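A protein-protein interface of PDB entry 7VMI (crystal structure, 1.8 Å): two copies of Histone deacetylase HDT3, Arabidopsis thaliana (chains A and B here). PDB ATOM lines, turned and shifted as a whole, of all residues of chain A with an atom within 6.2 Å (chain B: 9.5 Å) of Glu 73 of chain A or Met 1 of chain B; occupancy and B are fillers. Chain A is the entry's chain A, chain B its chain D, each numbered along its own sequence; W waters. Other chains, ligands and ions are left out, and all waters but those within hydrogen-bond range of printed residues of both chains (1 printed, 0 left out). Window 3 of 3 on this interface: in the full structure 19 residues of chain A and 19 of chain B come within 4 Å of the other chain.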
ATOM      1  N   ASP A  17      11.286  -9.659 -25.717  1.00  0.00           N
ATOM      2  CA  ASP A  17      10.131  -9.280 -24.936  1.00  0.00           C
ATOM      3  C   ASP A  17       8.910  -9.462 -25.825  1.00  0.00           C
ATOM      4  O   ASP A  17       8.826  -8.836 -26.867  1.00  0.00           O
ATOM      5  CB  ASP A  17      10.271  -7.832 -24.527  1.00  0.00           C
ATOM      6  CG  ASP A  17       9.165  -7.370 -23.638  1.00  0.00           C
ATOM      7  OD1 ASP A  17       8.142  -8.082 -23.453  1.00  0.00           O
ATOM      8  OD2 ASP A  17       9.377  -6.248 -23.120  1.00  0.00           O
ATOM      9  N   PRO A  18       7.922 -10.309 -25.463  1.00  0.00           N
ATOM     10  CA  PRO A  18       6.721 -10.468 -26.288  1.00  0.00           C
ATOM     11  C   PRO A  18       5.915  -9.170 -26.428  1.00  0.00           C
ATOM     12  O   PRO A  18       5.309  -8.972 -27.468  1.00  0.00           O
ATOM     13  CB  PRO A  18       5.875 -11.520 -25.545  1.00  0.00           C
ATOM     14  CG  PRO A  18       6.933 -12.239 -24.700  1.00  0.00           C
ATOM     15  CD  PRO A  18       7.904 -11.160 -24.267  1.00  0.00           C
ATOM     16  N   GLY A  19       5.949  -8.336 -25.379  1.00  0.00           N
ATOM     17  CA  GLY A  19       5.228  -7.095 -25.312  1.00  0.00           C
ATOM     18  C   GLY A  19       3.979  -7.266 -24.472  1.00  0.00           C
ATOM     19  O   GLY A  19       3.548  -8.383 -24.147  1.00  0.00           O
ATOM     20  N   ARG A  22       0.840  -9.827 -25.034  1.00  0.00           N
ATOM     21  CA  ARG A  22       1.243 -10.752 -26.118  1.00  0.00           C
ATOM     22  C   ARG A  22       2.011 -11.959 -25.576  1.00  0.00           C
ATOM     23  O   ARG A  22       2.586 -11.891 -24.483  1.00  0.00           O
ATOM     24  CB  ARG A  22       2.116 -10.027 -27.134  1.00  0.00           C
ATOM     25  CG  ARG A  22       1.393  -8.870 -27.798  1.00  0.00           C
ATOM     26  CD  ARG A  22       0.615  -9.445 -28.983  1.00  0.00           C
ATOM     27  NE  ARG A  22       0.152  -8.433 -29.920  1.00  0.00           N
ATOM     28  CZ  ARG A  22      -0.801  -7.533 -29.673  1.00  0.00           C
ATOM     29  NH1 ARG A  22      -1.425  -7.508 -28.504  1.00  0.00           N
ATOM     30  NH2 ARG A  22      -1.130  -6.648 -30.601  1.00  0.00           N
ATOM     31  N   LEU A  23       2.017 -13.022 -26.377  1.00  0.00           N
ATOM     32  CA  LEU A  23       2.826 -14.189 -26.150  1.00  0.00           C
ATOM     33  C   LEU A  23       3.663 -14.367 -27.400  1.00  0.00           C
ATOM     34  O   LEU A  23       3.210 -14.051 -28.503  1.00  0.00           O
ATOM     35  CB  LEU A  23       1.950 -15.436 -26.039  1.00  0.00           C
ATOM     36  CG  LEU A  23       0.828 -15.487 -25.008  1.00  0.00           C
ATOM     37  CD1 LEU A  23      -0.041 -16.708 -25.146  1.00  0.00           C
ATOM     38  CD2 LEU A  23       1.427 -15.455 -23.625  1.00  0.00           C
ATOM     39  N   VAL A  24       4.874 -14.899 -27.225  1.00  0.00           N
ATOM     40  CA  VAL A  24       5.605 -15.518 -28.327  1.00  0.00           C
ATOM     41  C   VAL A  24       5.406 -17.028 -28.214  1.00  0.00           C
ATOM     42  O   VAL A  24       5.625 -17.626 -27.154  1.00  0.00           O
ATOM     43  CB  VAL A  24       7.080 -15.137 -28.317  1.00  0.00           C
ATOM     44  CG1 VAL A  24       7.816 -15.930 -29.359  1.00  0.00           C
ATOM     45  CG2 VAL A  24       7.233 -13.652 -28.622  1.00  0.00           C
ATOM     46  N   HIS A  25       4.976 -17.632 -29.326  1.00  0.00           N
ATOM     47  CA  HIS A  25       4.822 -19.078 -29.505  1.00  0.00           C
ATOM     48  C   HIS A  25       5.904 -19.541 -30.469  1.00  0.00           C
ATOM     49  O   HIS A  25       5.877 -19.165 -31.650  1.00  0.00           O
ATOM     50  CB  HIS A  25       3.442 -19.307 -30.107  1.00  0.00           C
ATOM     51  CG  HIS A  25       3.014 -20.723 -30.135  1.00  0.00           C
ATOM     52  ND1 HIS A  25       3.676 -21.751 -30.798  1.00  0.00           N
ATOM     53  CD2 HIS A  25       1.899 -21.279 -29.607  1.00  0.00           C
ATOM     54  CE1 HIS A  25       2.993 -22.878 -30.647  1.00  0.00           C
ATOM     55  NE2 HIS A  25       1.913 -22.621 -29.927  1.00  0.00           N
ATOM     56  N   VAL A  48      14.197 -17.770 -18.763  1.00  0.00           N
ATOM     57  CA  VAL A  48      12.997 -16.953 -18.414  1.00  0.00           C
ATOM     58  C   VAL A  48      13.028 -16.676 -16.910  1.00  0.00           C
ATOM     59  O   VAL A  48      13.054 -17.653 -16.135  1.00  0.00           O
ATOM     60  CB  VAL A  48      11.690 -17.659 -18.824  1.00  0.00           C
ATOM     61  CG1 VAL A  48      10.509 -16.702 -18.826  1.00  0.00           C
ATOM     62  CG2 VAL A  48      11.815 -18.356 -20.170  1.00  0.00           C
ATOM     63  N   VAL A  71       5.913 -21.466 -25.230  1.00  0.00           N
ATOM     64  CA  VAL A  71       5.006 -20.345 -25.033  1.00  0.00           C
ATOM     65  C   VAL A  71       5.569 -19.389 -23.961  1.00  0.00           C
ATOM     66  O   VAL A  71       5.783 -19.776 -22.842  1.00  0.00           O
ATOM     67  CB  VAL A  71       3.603 -20.835 -24.702  1.00  0.00           C
ATOM     68  CG1 VAL A  71       2.673 -19.685 -24.297  1.00  0.00           C
ATOM     69  CG2 VAL A  71       3.024 -21.561 -25.925  1.00  0.00           C
ATOM     70  N   LEU A  72       5.792 -18.127 -24.359  1.00  0.00           N
ATOM     71  CA  LEU A  72       6.498 -17.140 -23.567  1.00  0.00           C
ATOM     72  C   LEU A  72       5.684 -15.858 -23.456  1.00  0.00           C
ATOM     73  O   LEU A  72       5.377 -15.203 -24.462  1.00  0.00           O
ATOM     74  CB  LEU A  72       7.831 -16.872 -24.231  1.00  0.00           C
ATOM     75  CG  LEU A  72       8.701 -18.130 -24.229  1.00  0.00           C
ATOM     76  CD1 LEU A  72       9.621 -18.110 -25.430  1.00  0.00           C
ATOM     77  CD2 LEU A  72       9.465 -18.299 -22.907  1.00  0.00           C
ATOM     78  N   GLU A  73       5.290 -15.511 -22.230  1.00  0.00           N
ATOM     79  CA  GLU A  73       4.435 -14.366 -21.983  1.00  0.00           C
ATOM     80  C   GLU A  73       5.249 -13.216 -21.416  1.00  0.00           C
ATOM     81  O   GLU A  73       4.755 -12.114 -21.284  1.00  0.00           O
ATOM     82  CB  GLU A  73       3.284 -14.722 -21.022  1.00  0.00           C
ATOM     83  CG  GLU A  73       3.569 -14.668 -19.540  1.00  0.00           C
ATOM     84  CD  GLU A  73       4.537 -15.720 -19.033  1.00  0.00           C
ATOM     85  OE1 GLU A  73       5.013 -16.569 -19.843  1.00  0.00           O
ATOM     86  OE2 GLU A  73       4.801 -15.677 -17.801  1.00  0.00           O
ATOM     87  N   ARG A  74       6.506 -13.479 -21.072  1.00  0.00           N
ATOM     88  CA  ARG A  74       7.360 -12.469 -20.412  1.00  0.00           C
ATOM     89  C   ARG A  74       8.740 -12.454 -21.062  1.00  0.00           C
ATOM     90  O   ARG A  74       9.001 -13.296 -21.936  1.00  0.00           O
ATOM     91  CB  ARG A  74       7.424 -12.775 -18.922  1.00  0.00           C
ATOM     92  CG  ARG A  74       7.994 -14.146 -18.605  1.00  0.00           C
ATOM     93  CD  ARG A  74       7.585 -14.471 -17.145  1.00  0.00           C
ATOM     94  NE  ARG A  74       8.150 -15.614 -16.421  1.00  0.00           N
ATOM     95  CZ  ARG A  74       7.579 -16.842 -16.325  1.00  0.00           C
ATOM     96  NH1 ARG A  74       6.430 -17.114 -16.931  1.00  0.00           N
ATOM     97  NH2 ARG A  74       8.217 -17.809 -15.690  1.00  0.00           N
ATOM     98  N   ASN A  75       9.573 -11.502 -20.650  1.00  0.00           N
ATOM     99  CA  ASN A  75      10.913 -11.351 -21.180  1.00  0.00           C
ATOM    100  C   ASN A  75      11.651 -12.676 -21.094  1.00  0.00           C
ATOM    101  O   ASN A  75      11.503 -13.410 -20.120  1.00  0.00           O
ATOM    102  CB  ASN A  75      11.706 -10.286 -20.399  1.00  0.00           C
ATOM    103  CG  ASN A  75      11.104  -8.899 -20.497  1.00  0.00           C
ATOM    104  OD1 ASN A  75      10.116  -8.658 -21.193  1.00  0.00           O
ATOM    105  ND2 ASN A  75      11.700  -7.983 -19.806  1.00  0.00           N
ATOM    106  N   PHE A  76      12.410 -12.996 -22.146  1.00  0.00           N
ATOM    107  CA  PHE A  76      13.217 -14.198 -22.180  1.00  0.00           C
ATOM    108  C   PHE A  76      14.430 -14.019 -23.053  1.00  0.00           C
ATOM    109  O   PHE A  76      14.545 -13.040 -23.778  1.00  0.00           O
ATOM    110  CB  PHE A  76      12.389 -15.391 -22.715  1.00  0.00           C
ATOM    111  CG  PHE A  76      11.924 -15.229 -24.120  1.00  0.00           C
ATOM    112  CD1 PHE A  76      10.798 -14.468 -24.428  1.00  0.00           C
ATOM    113  CD2 PHE A  76      12.596 -15.842 -25.146  1.00  0.00           C
ATOM    114  CE1 PHE A  76      10.356 -14.327 -25.726  1.00  0.00           C
ATOM    115  CE2 PHE A  76      12.160 -15.702 -26.467  1.00  0.00           C
ATOM    116  CZ  PHE A  76      11.045 -14.951 -26.761  1.00  0.00           C
ATOM    117  N   LEU A  96      -3.459 -11.569 -26.051  1.00  0.00           N
ATOM    118  CA  LEU A  96      -4.192 -11.947 -24.813  1.00  0.00           C
ATOM    119  C   LEU A  96      -3.484 -12.987 -23.965  1.00  0.00           C
ATOM    120  O   LEU A  96      -2.281 -13.114 -24.061  1.00  0.00           O
ATOM    121  CB  LEU A  96      -5.647 -12.443 -25.051  1.00  0.00           C
ATOM    122  CG  LEU A  96      -6.663 -11.428 -25.593  1.00  0.00           C
ATOM    123  CD1 LEU A  96      -6.841 -11.531 -27.106  1.00  0.00           C
ATOM    124  CD2 LEU A  96      -8.033 -11.565 -24.922  1.00  0.00           C
ATOM    125  N   MET B   1      -1.596 -18.228 -19.450  1.00  0.00           N
ATOM    126  CA  MET B   1      -0.390 -18.757 -20.176  1.00  0.00           C
ATOM    127  C   MET B   1       0.829 -18.197 -19.490  1.00  0.00           C
ATOM    128  O   MET B   1       1.161 -17.012 -19.624  1.00  0.00           O
ATOM    129  CB  MET B   1      -0.360 -18.317 -21.633  1.00  0.00           C
ATOM    130  CG  MET B   1      -1.507 -18.825 -22.486  1.00  0.00           C
ATOM    131  SD  MET B   1      -1.483 -20.601 -22.772  1.00  0.00           S
ATOM    132  CE  MET B   1      -0.848 -20.856 -24.421  1.00  0.00           C
ATOM    133  N   GLU B   2       1.521 -19.069 -18.764  1.00  0.00           N
ATOM    134  CA  GLU B   2       2.689 -18.704 -18.008  1.00  0.00           C
ATOM    135  C   GLU B   2       3.738 -19.735 -18.322  1.00  0.00           C
ATOM    136  O   GLU B   2       3.514 -20.903 -18.079  1.00  0.00           O
ATOM    137  CB  GLU B   2       2.315 -18.762 -16.561  1.00  0.00           C
ATOM    138  CG  GLU B   2       3.399 -18.399 -15.589  1.00  0.00           C
ATOM    139  CD  GLU B   2       2.927 -18.332 -14.153  1.00  0.00           C
ATOM    140  OE1 GLU B   2       1.847 -18.781 -13.812  1.00  0.00           O
ATOM    141  OE2 GLU B   2       3.682 -17.781 -13.341  1.00  0.00           O
ATOM    142  N   PHE B   3       4.892 -19.307 -18.847  1.00  0.00           N
ATOM    143  CA  PHE B   3       5.981 -20.242 -19.102  1.00  0.00           C
ATOM    144  C   PHE B   3       6.341 -20.979 -17.831  1.00  0.00           C
ATOM    145  O   PHE B   3       6.372 -20.404 -16.744  1.00  0.00           O
ATOM    146  CB  PHE B   3       7.218 -19.535 -19.640  1.00  0.00           C
ATOM    147  CG  PHE B   3       8.347 -20.455 -19.891  1.00  0.00           C
ATOM    148  CD1 PHE B   3       8.422 -21.180 -21.057  1.00  0.00           C
ATOM    149  CD2 PHE B   3       9.349 -20.642 -18.917  1.00  0.00           C
ATOM    150  CE1 PHE B   3       9.470 -22.078 -21.269  1.00  0.00           C
ATOM    151  CE2 PHE B   3      10.397 -21.513 -19.129  1.00  0.00           C
ATOM    152  CZ  PHE B   3      10.465 -22.223 -20.291  1.00  0.00           C
ATOM    153  N   TRP B   4       6.619 -22.273 -17.972  1.00  0.00           N
ATOM    154  CA  TRP B   4       6.888 -23.126 -16.837  1.00  0.00           C
ATOM    155  C   TRP B   4       7.987 -24.076 -17.258  1.00  0.00           C
ATOM    156  O   TRP B   4       7.998 -24.556 -18.407  1.00  0.00           O
ATOM    157  CB  TRP B   4       5.615 -23.928 -16.502  1.00  0.00           C
ATOM    158  CG  TRP B   4       5.833 -25.018 -15.519  1.00  0.00           C
ATOM    159  CD1 TRP B   4       5.750 -24.924 -14.148  1.00  0.00           C
ATOM    160  CD2 TRP B   4       6.193 -26.367 -15.802  1.00  0.00           C
ATOM    161  NE1 TRP B   4       6.057 -26.138 -13.585  1.00  0.00           N
ATOM    162  CE2 TRP B   4       6.311 -27.041 -14.575  1.00  0.00           C
ATOM    163  CE3 TRP B   4       6.453 -27.070 -16.974  1.00  0.00           C
ATOM    164  CZ2 TRP B   4       6.674 -28.392 -14.491  1.00  0.00           C
ATOM    165  CZ3 TRP B   4       6.839 -28.398 -16.883  1.00  0.00           C
ATOM    166  CH2 TRP B   4       6.935 -29.037 -15.662  1.00  0.00           C
ATOM    167  N   GLY B   5       8.892 -24.381 -16.325  1.00  0.00           N
ATOM    168  CA  GLY B   5       9.825 -25.450 -16.548  1.00  0.00           C
ATOM    169  C   GLY B   5      10.604 -25.874 -15.334  1.00  0.00           C
ATOM    170  O   GLY B   5      10.781 -25.096 -14.400  1.00  0.00           O
ATOM    171  N   ARG B  22      -5.758 -24.453 -12.197  1.00  0.00           N
ATOM    172  CA  ARG B  22      -4.673 -24.341 -13.199  1.00  0.00           C
ATOM    173  C   ARG B  22      -4.280 -25.726 -13.730  1.00  0.00           C
ATOM    174  O   ARG B  22      -4.541 -26.736 -13.070  1.00  0.00           O
ATOM    175  CB  ARG B  22      -3.445 -23.659 -12.588  1.00  0.00           C
ATOM    176  CG  ARG B  22      -3.758 -22.338 -11.910  1.00  0.00           C
ATOM    177  CD  ARG B  22      -2.544 -21.438 -11.877  1.00  0.00           C
ATOM    178  NE  ARG B  22      -2.366 -20.763 -13.159  1.00  0.00           N
ATOM    179  CZ  ARG B  22      -1.274 -20.087 -13.533  1.00  0.00           C
ATOM    180  NH1 ARG B  22      -0.228 -19.984 -12.730  1.00  0.00           N
ATOM    181  NH2 ARG B  22      -1.223 -19.508 -14.722  1.00  0.00           N
ATOM    182  N   LEU B  23      -3.640 -25.740 -14.896  1.00  0.00           N
ATOM    183  CA  LEU B  23      -3.109 -26.937 -15.503  1.00  0.00           C
ATOM    184  C   LEU B  23      -1.647 -26.658 -15.778  1.00  0.00           C
ATOM    185  O   LEU B  23      -1.303 -25.535 -16.094  1.00  0.00           O
ATOM    186  CB  LEU B  23      -3.755 -27.205 -16.867  1.00  0.00           C
ATOM    187  CG  LEU B  23      -5.233 -27.288 -17.030  1.00  0.00           C
ATOM    188  CD1 LEU B  23      -5.569 -27.350 -18.533  1.00  0.00           C
ATOM    189  CD2 LEU B  23      -5.749 -28.488 -16.256  1.00  0.00           C
ATOM    190  N   HIS B  25       0.877 -27.822 -18.680  1.00  0.00           N
ATOM    191  CA  HIS B  25       1.001 -28.370 -20.020  1.00  0.00           C
ATOM    192  C   HIS B  25       2.502 -28.524 -20.287  1.00  0.00           C
ATOM    193  O   HIS B  25       3.236 -27.537 -20.367  1.00  0.00           O
ATOM    194  CB  HIS B  25       0.367 -27.362 -21.009  1.00  0.00           C
ATOM    195  CG  HIS B  25       0.332 -27.823 -22.424  1.00  0.00           C
ATOM    196  ND1 HIS B  25      -0.853 -27.939 -23.141  1.00  0.00           N
ATOM    197  CD2 HIS B  25       1.327 -28.173 -23.284  1.00  0.00           C
ATOM    198  CE1 HIS B  25      -0.581 -28.353 -24.375  1.00  0.00           C
ATOM    199  NE2 HIS B  25       0.731 -28.514 -24.488  1.00  0.00           N
ATOM    200  N   SER B  27       5.328 -29.404 -22.807  1.00  0.00           N
ATOM    201  CA  SER B  27       5.502 -29.467 -24.240  1.00  0.00           C
ATOM    202  C   SER B  27       6.873 -29.950 -24.712  1.00  0.00           C
ATOM    203  O   SER B  27       7.002 -30.422 -25.858  1.00  0.00           O
ATOM    204  CB  SER B  27       5.196 -28.101 -24.881  1.00  0.00           C
ATOM    205  OG  SER B  27       6.029 -27.062 -24.352  1.00  0.00           O
ATOM    206  N   GLY B  91       7.147 -26.072 -20.539  1.00  0.00           N
ATOM    207  CA  GLY B  91       5.859 -25.856 -21.122  1.00  0.00           C
ATOM    208  C   GLY B  91       5.264 -24.609 -20.526  1.00  0.00           C
ATOM    209  O   GLY B  91       5.890 -23.552 -20.464  1.00  0.00           O
ATOM    210  N   TYR B  92       4.005 -24.708 -20.108  1.00  0.00           N
ATOM    211  CA  TYR B  92       3.254 -23.541 -19.606  1.00  0.00           C
ATOM    212  C   TYR B  92       2.092 -23.963 -18.707  1.00  0.00           C
ATOM    213  O   TYR B  92       1.579 -25.081 -18.834  1.00  0.00           O
ATOM    214  CB  TYR B  92       2.790 -22.676 -20.777  1.00  0.00           C
ATOM    215  CG  TYR B  92       2.032 -23.385 -21.874  1.00  0.00           C
ATOM    216  CD1 TYR B  92       0.649 -23.504 -21.835  1.00  0.00           C
ATOM    217  CD2 TYR B  92       2.692 -23.927 -22.964  1.00  0.00           C
ATOM    218  CE1 TYR B  92      -0.061 -24.137 -22.836  1.00  0.00           C
ATOM    219  CE2 TYR B  92       1.997 -24.570 -23.978  1.00  0.00           C
ATOM    220  CZ  TYR B  92       0.620 -24.655 -23.920  1.00  0.00           C
ATOM    221  OH  TYR B  92      -0.025 -25.285 -24.941  1.00  0.00           O
ATOM    222  N   LYS B  93       1.681 -23.038 -17.839  1.00  0.00           N
ATOM    223  CA  LYS B  93       0.505 -23.158 -17.018  1.00  0.00           C
ATOM    224  C   LYS B  93      -0.635 -22.390 -17.646  1.00  0.00           C
ATOM    225  O   LYS B  93      -0.437 -21.317 -18.228  1.00  0.00           O
ATOM    226  CB  LYS B  93       0.776 -22.600 -15.642  1.00  0.00           C
ATOM    227  CG  LYS B  93       1.787 -23.415 -14.854  1.00  0.00           C
ATOM    228  CD  LYS B  93       1.598 -23.157 -13.361  1.00  0.00           C
ATOM    229  CE  LYS B  93       2.538 -23.970 -12.503  1.00  0.00           C
ATOM    230  NZ  LYS B  93       2.183 -23.822 -11.072  1.00  0.00           N
ATOM    231  N   VAL B  94      -1.839 -22.948 -17.494  1.00  0.00           N
ATOM    232  CA  VAL B  94      -3.081 -22.448 -18.063  1.00  0.00           C
ATOM    233  C   VAL B  94      -4.078 -22.292 -16.936  1.00  0.00           C
ATOM    234  O   VAL B  94      -4.138 -23.118 -16.044  1.00  0.00           O
ATOM    235  CB  VAL B  94      -3.657 -23.491 -19.042  1.00  0.00           C
ATOM    236  CG1 VAL B  94      -4.877 -22.977 -19.753  1.00  0.00           C
ATOM    237  CG2 VAL B  94      -2.591 -23.897 -20.064  1.00  0.00           C
ATOM    238  N   ASP B  95      -4.884 -21.233 -16.985  1.00  0.00           N
ATOM    239  CA  ASP B  95      -5.990 -21.033 -16.046  1.00  0.00           C
ATOM    240  C   ASP B  95      -7.259 -21.634 -16.585  1.00  0.00           C
ATOM    241  O   ASP B  95      -7.499 -21.518 -17.771  1.00  0.00           O
ATOM    242  CB  ASP B  95      -6.203 -19.569 -15.795  1.00  0.00           C
ATOM    243  CG  ASP B  95      -5.663 -19.159 -14.464  1.00  0.00           C
ATOM    244  OD1 ASP B  95      -4.428 -19.250 -14.259  1.00  0.00           O
ATOM    245  OD2 ASP B  95      -6.493 -18.803 -13.612  1.00  0.00           O
ATOM    246  N   LEU B  96      -8.079 -22.220 -15.707  1.00  0.00           N
ATOM    247  CA  LEU B  96      -9.344 -22.867 -16.122  1.00  0.00           C
ATOM    248  C   LEU B  96     -10.558 -21.935 -16.134  1.00  0.00           C
ATOM    249  O   LEU B  96     -10.513 -20.798 -15.651  1.00  0.00           O
ATOM    250  CB  LEU B  96      -9.598 -24.149 -15.318  1.00  0.00           C
ATOM    251  CG  LEU B  96      -8.536 -25.217 -15.524  1.00  0.00           C
ATOM    252  CD1 LEU B  96      -8.894 -26.438 -14.697  1.00  0.00           C
ATOM    253  CD2 LEU B  96      -8.394 -25.594 -16.994  1.00  0.00           C
HETATM  254  O   HOH W   1       6.703 -23.308 -23.185  1.00  0.00           O
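The side-chain carboxylate (OE1) of Glu 73 of chain A lies within hydrogen-bond range of the backbone NH (N) of Phe 3 of chain B, 2.9 Å away.
The backbone carbonyl oxygen (O) of Phe 3 of chain B sits at hydrogen-bond distance from the guanidinium group (NH1) of Arg 74 of chain A (3.3 Å).
The backbone NH (N) of Val 24 of chain A sits at hydrogen-bond distance from the backbone carbonyl oxygen (O) of Leu 72 of chain A (2.8 Å).
The side-chain carboxylate (OE1) of Glu 73 of chain A lies within salt-bridge range of the guanidinium group (NH1) of Arg 74 of chain A (3.3 Å).
OE1 of Glu 2 of chain B is in salt-bridge range of NH1 of Arg 22 of chain B, at 2.6 Å.
O of Glu 2 of chain B lies within hydrogen-bond range of N of Lys 93 of chain B (2.8 Å).
The backbone carbonyl oxygen (O) of Tyr 92 of chain B lies within hydrogen-bond range of the backbone NH (N) of His 25 of chain B (2.8 Å).
Among the printed residues, pairs that only touch across the chains: Leu 23 of chain A with Met 1 of chain B (3.7 Å), Val 48 of chain A with Phe 3 of chain B (3.6 Å), Val 71 of chain A with Met 1 of chain B (3.7 Å), Val 71 of chain A with Phe 3 of chain B (3.5 Å), Val 71 of chain A with Tyr 92 of chain B (3.7 Å), Leu 72 of chain A with Phe 3 of chain B (3.6 Å), Glu 73 of chain A with Met 1 of chain B (3.4 Å), Glu 73 of chain A with Glu 2 of chain B (3.7 Å) and Arg 74 of chain A with Glu 2 of chain B (3.6 Å).
Glu 73 of chain A touches just these residues of chain B: Met 1 (3.4 Å), Glu 2 (3.7 Å) and Phe 3 (2.9 Å).
Met 1 of chain B touches three residues of chain A.
Arg 74 of chain A touches just these residues of chain B: Glu 2 (3.6 Å) and Phe 3 (3.3 Å).
Of the printed residues of chain B, Leu 23 of chain A touches Met 1.
Printed residues of chain A within 4 Å of Tyr 92 of chain B: Val 71.
Of the printed residues of chain A, Phe 3 of chain B touches Val 48 (3.6 Å), Val 71 (3.5 Å), Leu 72 (3.6 Å), Glu 73 (2.9 Å) and Arg 74 (3.3 Å).
The nearest residue of chain B that does not touch Glu 73 of chain A is Trp 4 of chain B (6.2 Å).
The nearest printed residue of chain A that does not touch Tyr 92 of chain B is His 25 of chain A (6.0 Å).
Of the 15 printed residues of chain B, 4 touch a printed residue of chain A.
Among the printed residues, 11 pairs touch across the chains.
4 positions are printed for both chains.
Of the 11 pairs that touch across the chains among the printed residues, none has its exchanged pair printed and touching as well.
Water W1 lies within hydrogen-bond range of O of Gly 91 of chain B (2.9 Å) and N of Val 71 of chain A (2.9 Å).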
